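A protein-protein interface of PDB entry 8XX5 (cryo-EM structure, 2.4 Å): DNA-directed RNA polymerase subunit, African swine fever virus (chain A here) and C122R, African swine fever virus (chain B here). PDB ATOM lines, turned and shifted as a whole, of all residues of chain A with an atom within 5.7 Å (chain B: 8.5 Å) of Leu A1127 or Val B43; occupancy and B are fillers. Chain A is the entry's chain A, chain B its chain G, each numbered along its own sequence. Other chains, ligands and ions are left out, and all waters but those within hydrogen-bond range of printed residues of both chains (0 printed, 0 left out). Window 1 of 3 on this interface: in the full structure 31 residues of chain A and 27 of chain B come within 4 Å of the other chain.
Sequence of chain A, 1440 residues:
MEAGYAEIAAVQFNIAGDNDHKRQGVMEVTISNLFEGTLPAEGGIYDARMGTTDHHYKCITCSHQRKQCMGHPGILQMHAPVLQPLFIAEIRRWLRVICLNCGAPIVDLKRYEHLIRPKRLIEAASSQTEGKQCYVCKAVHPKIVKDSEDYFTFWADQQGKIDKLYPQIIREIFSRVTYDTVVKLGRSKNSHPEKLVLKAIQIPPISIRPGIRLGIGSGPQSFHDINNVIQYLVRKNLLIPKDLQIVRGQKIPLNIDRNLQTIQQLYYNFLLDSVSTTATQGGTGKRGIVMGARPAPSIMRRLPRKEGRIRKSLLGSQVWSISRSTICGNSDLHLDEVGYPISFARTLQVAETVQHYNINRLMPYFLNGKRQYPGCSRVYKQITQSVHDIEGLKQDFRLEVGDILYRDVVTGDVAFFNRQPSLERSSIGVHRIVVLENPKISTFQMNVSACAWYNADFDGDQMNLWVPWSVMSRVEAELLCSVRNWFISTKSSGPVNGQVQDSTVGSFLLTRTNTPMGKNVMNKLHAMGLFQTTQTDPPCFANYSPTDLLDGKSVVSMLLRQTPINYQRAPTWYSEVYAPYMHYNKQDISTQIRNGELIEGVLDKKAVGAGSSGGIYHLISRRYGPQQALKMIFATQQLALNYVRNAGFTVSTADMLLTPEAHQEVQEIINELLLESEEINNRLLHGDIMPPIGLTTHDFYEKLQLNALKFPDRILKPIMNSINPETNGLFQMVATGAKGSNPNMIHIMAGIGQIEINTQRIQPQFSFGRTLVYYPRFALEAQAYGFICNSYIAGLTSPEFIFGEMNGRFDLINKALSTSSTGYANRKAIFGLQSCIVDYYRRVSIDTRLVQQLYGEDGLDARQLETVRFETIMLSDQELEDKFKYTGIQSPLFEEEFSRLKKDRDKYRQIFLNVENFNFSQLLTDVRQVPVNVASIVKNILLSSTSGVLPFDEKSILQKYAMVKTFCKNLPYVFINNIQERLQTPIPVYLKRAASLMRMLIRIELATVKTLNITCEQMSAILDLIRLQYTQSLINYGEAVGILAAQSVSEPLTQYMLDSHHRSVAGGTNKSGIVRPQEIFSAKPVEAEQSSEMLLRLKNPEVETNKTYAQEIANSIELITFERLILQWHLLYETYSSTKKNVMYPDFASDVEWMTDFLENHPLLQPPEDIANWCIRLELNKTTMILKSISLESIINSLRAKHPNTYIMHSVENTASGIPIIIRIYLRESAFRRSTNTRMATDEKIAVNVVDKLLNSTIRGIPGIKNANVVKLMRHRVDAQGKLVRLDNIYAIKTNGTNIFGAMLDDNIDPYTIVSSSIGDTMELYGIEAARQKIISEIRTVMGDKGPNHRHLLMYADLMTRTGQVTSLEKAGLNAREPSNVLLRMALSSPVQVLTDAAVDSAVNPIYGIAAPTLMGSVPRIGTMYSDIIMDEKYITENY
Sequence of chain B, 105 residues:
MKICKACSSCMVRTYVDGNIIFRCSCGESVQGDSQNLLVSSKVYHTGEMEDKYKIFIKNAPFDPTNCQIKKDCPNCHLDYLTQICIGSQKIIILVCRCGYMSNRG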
ATOM      1  N   LEU A1125     -28.582 -21.679 -33.874  1.00  0.00           N
ATOM      2  CA  LEU A1125     -28.146 -22.659 -32.893  1.00  0.00           C
ATOM      3  C   LEU A1125     -26.657 -22.570 -32.579  1.00  0.00           C
ATOM      4  O   LEU A1125     -26.123 -23.471 -31.925  1.00  0.00           O
ATOM      5  CB  LEU A1125     -28.501 -24.067 -33.382  1.00  0.00           C
ATOM      6  CG  LEU A1125     -29.758 -24.166 -34.257  1.00  0.00           C
ATOM      7  CD1 LEU A1125     -29.996 -25.582 -34.670  1.00  0.00           C
ATOM      8  CD2 LEU A1125     -31.004 -23.653 -33.555  1.00  0.00           C
ATOM      9  N   ILE A1126     -25.978 -21.522 -33.034  1.00  0.00           N
ATOM     10  CA  ILE A1126     -24.550 -21.346 -32.798  1.00  0.00           C
ATOM     11  C   ILE A1126     -24.343 -20.392 -31.631  1.00  0.00           C
ATOM     12  O   ILE A1126     -24.876 -19.277 -31.624  1.00  0.00           O
ATOM     13  CB  ILE A1126     -23.844 -20.824 -34.061  1.00  0.00           C
ATOM     14  CG1 ILE A1126     -23.812 -21.901 -35.142  1.00  0.00           C
ATOM     15  CG2 ILE A1126     -22.431 -20.373 -33.736  1.00  0.00           C
ATOM     16  CD1 ILE A1126     -23.535 -23.280 -34.608  1.00  0.00           C
ATOM     17  N   LEU A1127     -23.573 -20.834 -30.636  1.00  0.00           N
ATOM     18  CA  LEU A1127     -23.126 -19.924 -29.590  1.00  0.00           C
ATOM     19  C   LEU A1127     -21.954 -19.081 -30.078  1.00  0.00           C
ATOM     20  O   LEU A1127     -21.960 -17.853 -29.938  1.00  0.00           O
ATOM     21  CB  LEU A1127     -22.741 -20.707 -28.335  1.00  0.00           C
ATOM     22  CG  LEU A1127     -23.669 -20.547 -27.131  1.00  0.00           C
ATOM     23  CD1 LEU A1127     -23.231 -21.456 -25.998  1.00  0.00           C
ATOM     24  CD2 LEU A1127     -23.703 -19.098 -26.675  1.00  0.00           C
ATOM     25  N   GLN A1128     -20.945 -19.727 -30.655  1.00  0.00           N
ATOM     26  CA  GLN A1128     -19.833 -19.036 -31.290  1.00  0.00           C
ATOM     27  C   GLN A1128     -19.199 -19.983 -32.298  1.00  0.00           C
ATOM     28  O   GLN A1128     -19.366 -21.202 -32.217  1.00  0.00           O
ATOM     29  CB  GLN A1128     -18.802 -18.553 -30.266  1.00  0.00           C
ATOM     30  CG  GLN A1128     -17.718 -19.561 -29.936  1.00  0.00           C
ATOM     31  CD  GLN A1128     -17.826 -20.091 -28.522  1.00  0.00           C
ATOM     32  OE1 GLN A1128     -18.882 -20.560 -28.100  1.00  0.00           O
ATOM     33  NE2 GLN A1128     -16.729 -20.019 -27.779  1.00  0.00           N
ATOM     34  N   TRP A1129     -18.480 -19.408 -33.258  1.00  0.00           N
ATOM     35  CA  TRP A1129     -17.800 -20.203 -34.271  1.00  0.00           C
ATOM     36  C   TRP A1129     -16.404 -19.649 -34.504  1.00  0.00           C
ATOM     37  O   TRP A1129     -16.174 -18.440 -34.416  1.00  0.00           O
ATOM     38  CB  TRP A1129     -18.570 -20.238 -35.598  1.00  0.00           C
ATOM     39  CG  TRP A1129     -18.757 -18.897 -36.227  1.00  0.00           C
ATOM     40  CD1 TRP A1129     -19.811 -18.054 -36.059  1.00  0.00           C
ATOM     41  CD2 TRP A1129     -17.862 -18.244 -37.136  1.00  0.00           C
ATOM     42  NE1 TRP A1129     -19.631 -16.915 -36.802  1.00  0.00           N
ATOM     43  CE2 TRP A1129     -18.440 -17.007 -37.472  1.00  0.00           C
ATOM     44  CE3 TRP A1129     -16.627 -18.587 -37.694  1.00  0.00           C
ATOM     45  CZ2 TRP A1129     -17.826 -16.109 -38.341  1.00  0.00           C
ATOM     46  CZ3 TRP A1129     -16.020 -17.696 -38.555  1.00  0.00           C
ATOM     47  CH2 TRP A1129     -16.619 -16.472 -38.871  1.00  0.00           C
ATOM     48  N   HIS A1130     -15.478 -20.551 -34.821  1.00  0.00           N
ATOM     49  CA  HIS A1130     -14.090 -20.193 -35.090  1.00  0.00           C
ATOM     50  C   HIS A1130     -13.635 -20.918 -36.347  1.00  0.00           C
ATOM     51  O   HIS A1130     -13.693 -22.149 -36.409  1.00  0.00           O
ATOM     52  CB  HIS A1130     -13.187 -20.559 -33.910  1.00  0.00           C
ATOM     53  CG  HIS A1130     -13.487 -19.794 -32.661  1.00  0.00           C
ATOM     54  ND1 HIS A1130     -13.331 -20.330 -31.403  1.00  0.00           N
ATOM     55  CD2 HIS A1130     -13.930 -18.529 -32.477  1.00  0.00           C
ATOM     56  CE1 HIS A1130     -13.667 -19.431 -30.497  1.00  0.00           C
ATOM     57  NE2 HIS A1130     -14.035 -18.328 -31.123  1.00  0.00           N
ATOM     58  N   GLU A1179     -19.575 -23.822 -31.678  1.00  0.00           N
ATOM     59  CA  GLU A1179     -20.142 -24.302 -30.426  1.00  0.00           C
ATOM     60  C   GLU A1179     -21.662 -24.220 -30.512  1.00  0.00           C
ATOM     61  O   GLU A1179     -22.217 -23.145 -30.763  1.00  0.00           O
ATOM     62  CB  GLU A1179     -19.621 -23.483 -29.246  1.00  0.00           C
ATOM     63  CG  GLU A1179     -18.176 -23.768 -28.855  1.00  0.00           C
ATOM     64  CD  GLU A1179     -17.157 -23.058 -29.730  1.00  0.00           C
ATOM     65  OE1 GLU A1179     -17.495 -22.667 -30.865  1.00  0.00           O
ATOM     66  OE2 GLU A1179     -16.007 -22.886 -29.276  1.00  0.00           O
ATOM     67  N   LEU A1180     -22.327 -25.352 -30.308  1.00  0.00           N
ATOM     68  CA  LEU A1180     -23.780 -25.393 -30.361  1.00  0.00           C
ATOM     69  C   LEU A1180     -24.372 -24.870 -29.059  1.00  0.00           C
ATOM     70  O   LEU A1180     -23.879 -25.174 -27.969  1.00  0.00           O
ATOM     71  CB  LEU A1180     -24.269 -26.820 -30.619  1.00  0.00           C
ATOM     72  CG  LEU A1180     -23.832 -27.510 -31.914  1.00  0.00           C
ATOM     73  CD1 LEU A1180     -24.828 -28.587 -32.309  1.00  0.00           C
ATOM     74  CD2 LEU A1180     -23.660 -26.508 -33.043  1.00  0.00           C
ATOM     75  N   ASN A1181     -25.434 -24.077 -29.178  1.00  0.00           N
ATOM     76  CA  ASN A1181     -26.158 -23.579 -28.015  1.00  0.00           C
ATOM     77  C   ASN A1181     -27.128 -24.660 -27.552  1.00  0.00           C
ATOM     78  O   ASN A1181     -28.083 -24.992 -28.261  1.00  0.00           O
ATOM     79  CB  ASN A1181     -26.890 -22.283 -28.352  1.00  0.00           C
ATOM     80  CG  ASN A1181     -27.502 -21.620 -27.131  1.00  0.00           C
ATOM     81  OD1 ASN A1181     -27.116 -21.906 -25.999  1.00  0.00           O
ATOM     82  ND2 ASN A1181     -28.463 -20.732 -27.356  1.00  0.00           N
ATOM     83  N   LYS A1182     -26.880 -25.217 -26.364  1.00  0.00           N
ATOM     84  CA  LYS A1182     -27.705 -26.319 -25.883  1.00  0.00           C
ATOM     85  C   LYS A1182     -29.081 -25.831 -25.439  1.00  0.00           C
ATOM     86  O   LYS A1182     -30.072 -26.550 -25.599  1.00  0.00           O
ATOM     87  CB  LYS A1182     -26.988 -27.040 -24.739  1.00  0.00           C
ATOM     88  CG  LYS A1182     -27.528 -28.428 -24.373  1.00  0.00           C
ATOM     89  CD  LYS A1182     -28.357 -29.066 -25.483  1.00  0.00           C
ATOM     90  CE  LYS A1182     -28.646 -30.530 -25.193  1.00  0.00           C
ATOM     91  NZ  LYS A1182     -29.478 -31.148 -26.262  1.00  0.00           N
ATOM     92  N   SER B  40     -10.848 -16.139 -37.739  1.00  0.00           N
ATOM     93  CA  SER B  40     -12.073 -15.385 -37.516  1.00  0.00           C
ATOM     94  C   SER B  40     -12.818 -15.929 -36.305  1.00  0.00           C
ATOM     95  O   SER B  40     -12.809 -17.133 -36.035  1.00  0.00           O
ATOM     96  CB  SER B  40     -12.986 -15.420 -38.748  1.00  0.00           C
ATOM     97  OG  SER B  40     -13.011 -16.712 -39.327  1.00  0.00           O
ATOM     98  N   SER B  41     -13.474 -15.020 -35.586  1.00  0.00           N
ATOM     99  CA  SER B  41     -14.210 -15.344 -34.373  1.00  0.00           C
ATOM    100  C   SER B  41     -15.508 -14.551 -34.356  1.00  0.00           C
ATOM    101  O   SER B  41     -15.544 -13.405 -34.813  1.00  0.00           O
ATOM    102  CB  SER B  41     -13.384 -15.026 -33.122  1.00  0.00           C
ATOM    103  OG  SER B  41     -13.906 -15.669 -31.974  1.00  0.00           O
ATOM    104  N   LYS B  42     -16.568 -15.161 -33.832  1.00  0.00           N
ATOM    105  CA  LYS B  42     -17.842 -14.462 -33.679  1.00  0.00           C
ATOM    106  C   LYS B  42     -18.675 -15.236 -32.670  1.00  0.00           C
ATOM    107  O   LYS B  42     -18.992 -16.407 -32.903  1.00  0.00           O
ATOM    108  CB  LYS B  42     -18.564 -14.342 -35.032  1.00  0.00           C
ATOM    109  CG  LYS B  42     -20.093 -14.171 -35.011  1.00  0.00           C
ATOM    110  CD  LYS B  42     -20.576 -13.115 -34.015  1.00  0.00           C
ATOM    111  CE  LYS B  42     -21.648 -12.226 -34.619  1.00  0.00           C
ATOM    112  NZ  LYS B  42     -22.404 -11.485 -33.571  1.00  0.00           N
ATOM    113  N   VAL B  43     -19.029 -14.589 -31.561  1.00  0.00           N
ATOM    114  CA  VAL B  43     -19.941 -15.149 -30.569  1.00  0.00           C
ATOM    115  C   VAL B  43     -21.320 -14.559 -30.814  1.00  0.00           C
ATOM    116  O   VAL B  43     -21.479 -13.333 -30.866  1.00  0.00           O
ATOM    117  CB  VAL B  43     -19.456 -14.861 -29.138  1.00  0.00           C
ATOM    118  CG1 VAL B  43     -20.191 -15.742 -28.142  1.00  0.00           C
ATOM    119  CG2 VAL B  43     -17.955 -15.077 -29.036  1.00  0.00           C
ATOM    120  N   TYR B  44     -22.320 -15.426 -30.971  1.00  0.00           N
ATOM    121  CA  TYR B  44     -23.626 -15.008 -31.463  1.00  0.00           C
ATOM    122  C   TYR B  44     -24.620 -14.658 -30.366  1.00  0.00           C
ATOM    123  O   TYR B  44     -25.689 -14.122 -30.677  1.00  0.00           O
ATOM    124  CB  TYR B  44     -24.225 -16.100 -32.354  1.00  0.00           C
ATOM    125  CG  TYR B  44     -23.855 -15.947 -33.808  1.00  0.00           C
ATOM    126  CD1 TYR B  44     -24.221 -14.813 -34.520  1.00  0.00           C
ATOM    127  CD2 TYR B  44     -23.134 -16.930 -34.467  1.00  0.00           C
ATOM    128  CE1 TYR B  44     -23.881 -14.666 -35.848  1.00  0.00           C
ATOM    129  CE2 TYR B  44     -22.793 -16.794 -35.794  1.00  0.00           C
ATOM    130  CZ  TYR B  44     -23.163 -15.659 -36.479  1.00  0.00           C
ATOM    131  OH  TYR B  44     -22.824 -15.522 -37.805  1.00  0.00           O
ATOM    132  N   HIS B  45     -24.308 -14.934 -29.105  1.00  0.00           N
ATOM    133  CA  HIS B  45     -25.209 -14.632 -27.999  1.00  0.00           C
ATOM    134  C   HIS B  45     -24.617 -13.581 -27.068  1.00  0.00           C
ATOM    135  O   HIS B  45     -24.816 -13.618 -25.853  1.00  0.00           O
ATOM    136  CB  HIS B  45     -25.571 -15.899 -27.228  1.00  0.00           C
ATOM    137  CG  HIS B  45     -26.812 -16.568 -27.727  1.00  0.00           C
ATOM    138  ND1 HIS B  45     -27.948 -15.867 -28.069  1.00  0.00           N
ATOM    139  CD2 HIS B  45     -27.096 -17.873 -27.948  1.00  0.00           C
ATOM    140  CE1 HIS B  45     -28.878 -16.710 -28.476  1.00  0.00           C
ATOM    141  NE2 HIS B  45     -28.388 -17.934 -28.412  1.00  0.00           N
ATOM    142  N   THR B  46     -23.879 -12.633 -27.636  1.00  0.00           N
ATOM    143  CA  THR B  46     -23.387 -11.510 -26.856  1.00  0.00           C
ATOM    144  C   THR B  46     -24.549 -10.628 -26.417  1.00  0.00           C
ATOM    145  O   THR B  46     -25.599 -10.567 -27.066  1.00  0.00           O
ATOM    146  CB  THR B  46     -22.373 -10.697 -27.657  1.00  0.00           C
ATOM    147  OG1 THR B  46     -23.027 -10.074 -28.769  1.00  0.00           O
ATOM    148  CG2 THR B  46     -21.254 -11.595 -28.164  1.00  0.00           C
ATOM    149  N   GLY B  47     -24.356  -9.942 -25.294  1.00  0.00           N
ATOM    150  CA  GLY B  47     -25.437  -9.278 -24.607  1.00  0.00           C
ATOM    151  C   GLY B  47     -26.144 -10.148 -23.594  1.00  0.00           C
ATOM    152  O   GLY B  47     -27.007  -9.648 -22.860  1.00  0.00           O
ATOM    153  N   GLU B  48     -25.814 -11.439 -23.542  1.00  0.00           N
ATOM    154  CA  GLU B  48     -26.389 -12.364 -22.578  1.00  0.00           C
ATOM    155  C   GLU B  48     -25.341 -13.301 -21.992  1.00  0.00           C
ATOM    156  O   GLU B  48     -25.702 -14.272 -21.318  1.00  0.00           O
ATOM    157  CB  GLU B  48     -27.519 -13.174 -23.225  1.00  0.00           C
ATOM    158  CG  GLU B  48     -28.726 -13.390 -22.330  1.00  0.00           C
ATOM    159  CD  GLU B  48     -28.646 -14.682 -21.540  1.00  0.00           C
ATOM    160  OE1 GLU B  48     -28.408 -15.740 -22.160  1.00  0.00           O
ATOM    161  OE2 GLU B  48     -28.824 -14.641 -20.305  1.00  0.00           O
ATOM    162  N   MET B  49     -24.057 -13.042 -22.222  1.00  0.00           N
ATOM    163  CA  MET B  49     -23.030 -13.936 -21.716  1.00  0.00           C
ATOM    164  C   MET B  49     -22.788 -13.671 -20.231  1.00  0.00           C
ATOM    165  O   MET B  49     -23.410 -12.806 -19.610  1.00  0.00           O
ATOM    166  CB  MET B  49     -21.741 -13.785 -22.519  1.00  0.00           C
ATOM    167  CG  MET B  49     -20.966 -12.519 -22.222  1.00  0.00           C
ATOM    168  SD  MET B  49     -20.322 -11.746 -23.714  1.00  0.00           S
ATOM    169  CE  MET B  49     -21.508 -10.430 -23.929  1.00  0.00           C
ATOM    170  N   ASP B  51     -19.828 -12.675 -18.787  1.00  0.00           N
ATOM    171  CA  ASP B  51     -19.002 -11.510 -18.496  1.00  0.00           C
ATOM    172  C   ASP B  51     -19.718 -10.199 -18.788  1.00  0.00           C
ATOM    173  O   ASP B  51     -19.226  -9.140 -18.385  1.00  0.00           O
ATOM    174  CB  ASP B  51     -17.686 -11.573 -19.278  1.00  0.00           C
ATOM    175  CG  ASP B  51     -17.892 -11.837 -20.754  1.00  0.00           C
ATOM    176  OD1 ASP B  51     -18.128 -13.008 -21.120  1.00  0.00           O
ATOM    177  OD2 ASP B  51     -17.818 -10.876 -21.549  1.00  0.00           O
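Among the printed residues, merely in contact across the chains: Gln A1128 with Lys B42 (3.2 Å), Trp A1129 with Tyr B44 (3.2 Å), Trp A1129 with Ser B40 (3.3 Å), Leu A1127 with Val B43 (3.3 Å), Ile A1126 with Tyr B44 (3.3 Å), His A1130 with Ser B40 (3.4 Å), Gln A1128 with Val B43 (3.6 Å), Trp A1129 with Ser B41 (3.7 Å) and Leu A1127 with His B45 (3.7 Å).
A ring nitrogen (NE2) of His A1130 is in hydrogen-bond range of the side-chain hydroxyl (OG) of Ser B41 (2.8 Å).
The backbone carbonyl oxygen of Lys B42 lies within hydrogen-bond range of the backbone NH of Trp A1129 (3.1 Å).
The backbone NH (N) of Tyr B44 lies within hydrogen-bond range of the backbone carbonyl oxygen (O) of Leu A1127 (2.7 Å).
NE2 of His B45 is in hydrogen-bond range of ND2 of Asn A1181, at 3.0 Å.
Leu A1127 touches three residues of chain B.
Of chain A, only Leu A1127 (3.3 Å) and Gln A1128 (3.6 Å) come within 4 Å of Val B43.
Printed residues of chain A within 4 Å of Tyr B44: Ile A1126, Leu A1127 and Trp A1129.
Printed residues of chain A within 4 Å of His B45: Leu A1127 and Asn A1181.
Thr B46 touches none of the printed residues of chain A.
The nearest residue of chain B that does not touch Leu A1127 is Lys B42 (4.4 Å).
The nearest residue of chain A that does not touch Val B43 is Trp A1129 (5.1 Å).
The nearest printed residue of chain A that does not touch Ser B40 is Gln A1128 (7.9 Å).
Of the 10 printed residues of chain A, 6 touch a printed residue of chain B.
Hydrophobic or aromatic side chains of chain A within 4 Å of the printed part of chain B: Ile A1126, Leu A1127, Trp A1129 and His A1130.
Printed residues of chain B that touch a printed residue of chain A: Ser B40, Ser B41, Lys B42, Val B43, Tyr B44 and His B45.
Hydrophobic or aromatic side chains of chain B that line the printed part of chain A: Val B43, Tyr B44 and His B45.
Along chain B the printed residues that touch a printed residue of chain A span positions 40 to 45.
Among the printed residues, no Asp or Glu carboxylate lies within 4 Å of a Lys or Arg side-chain nitrogen of the other chain.
The backbone carbonyl oxygen (O) of Leu A1125 lies within hydrogen-bond range of the backbone NH (N) of Asn A1181 (2.9 Å).
The backbone carbonyl oxygen of Glu A1179 sits at hydrogen-bond distance from the backbone NH of Leu A1127 (2.7 Å).
The backbone NH of Glu A1179 sits at hydrogen-bond distance from the backbone carbonyl oxygen of Gln A1128.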
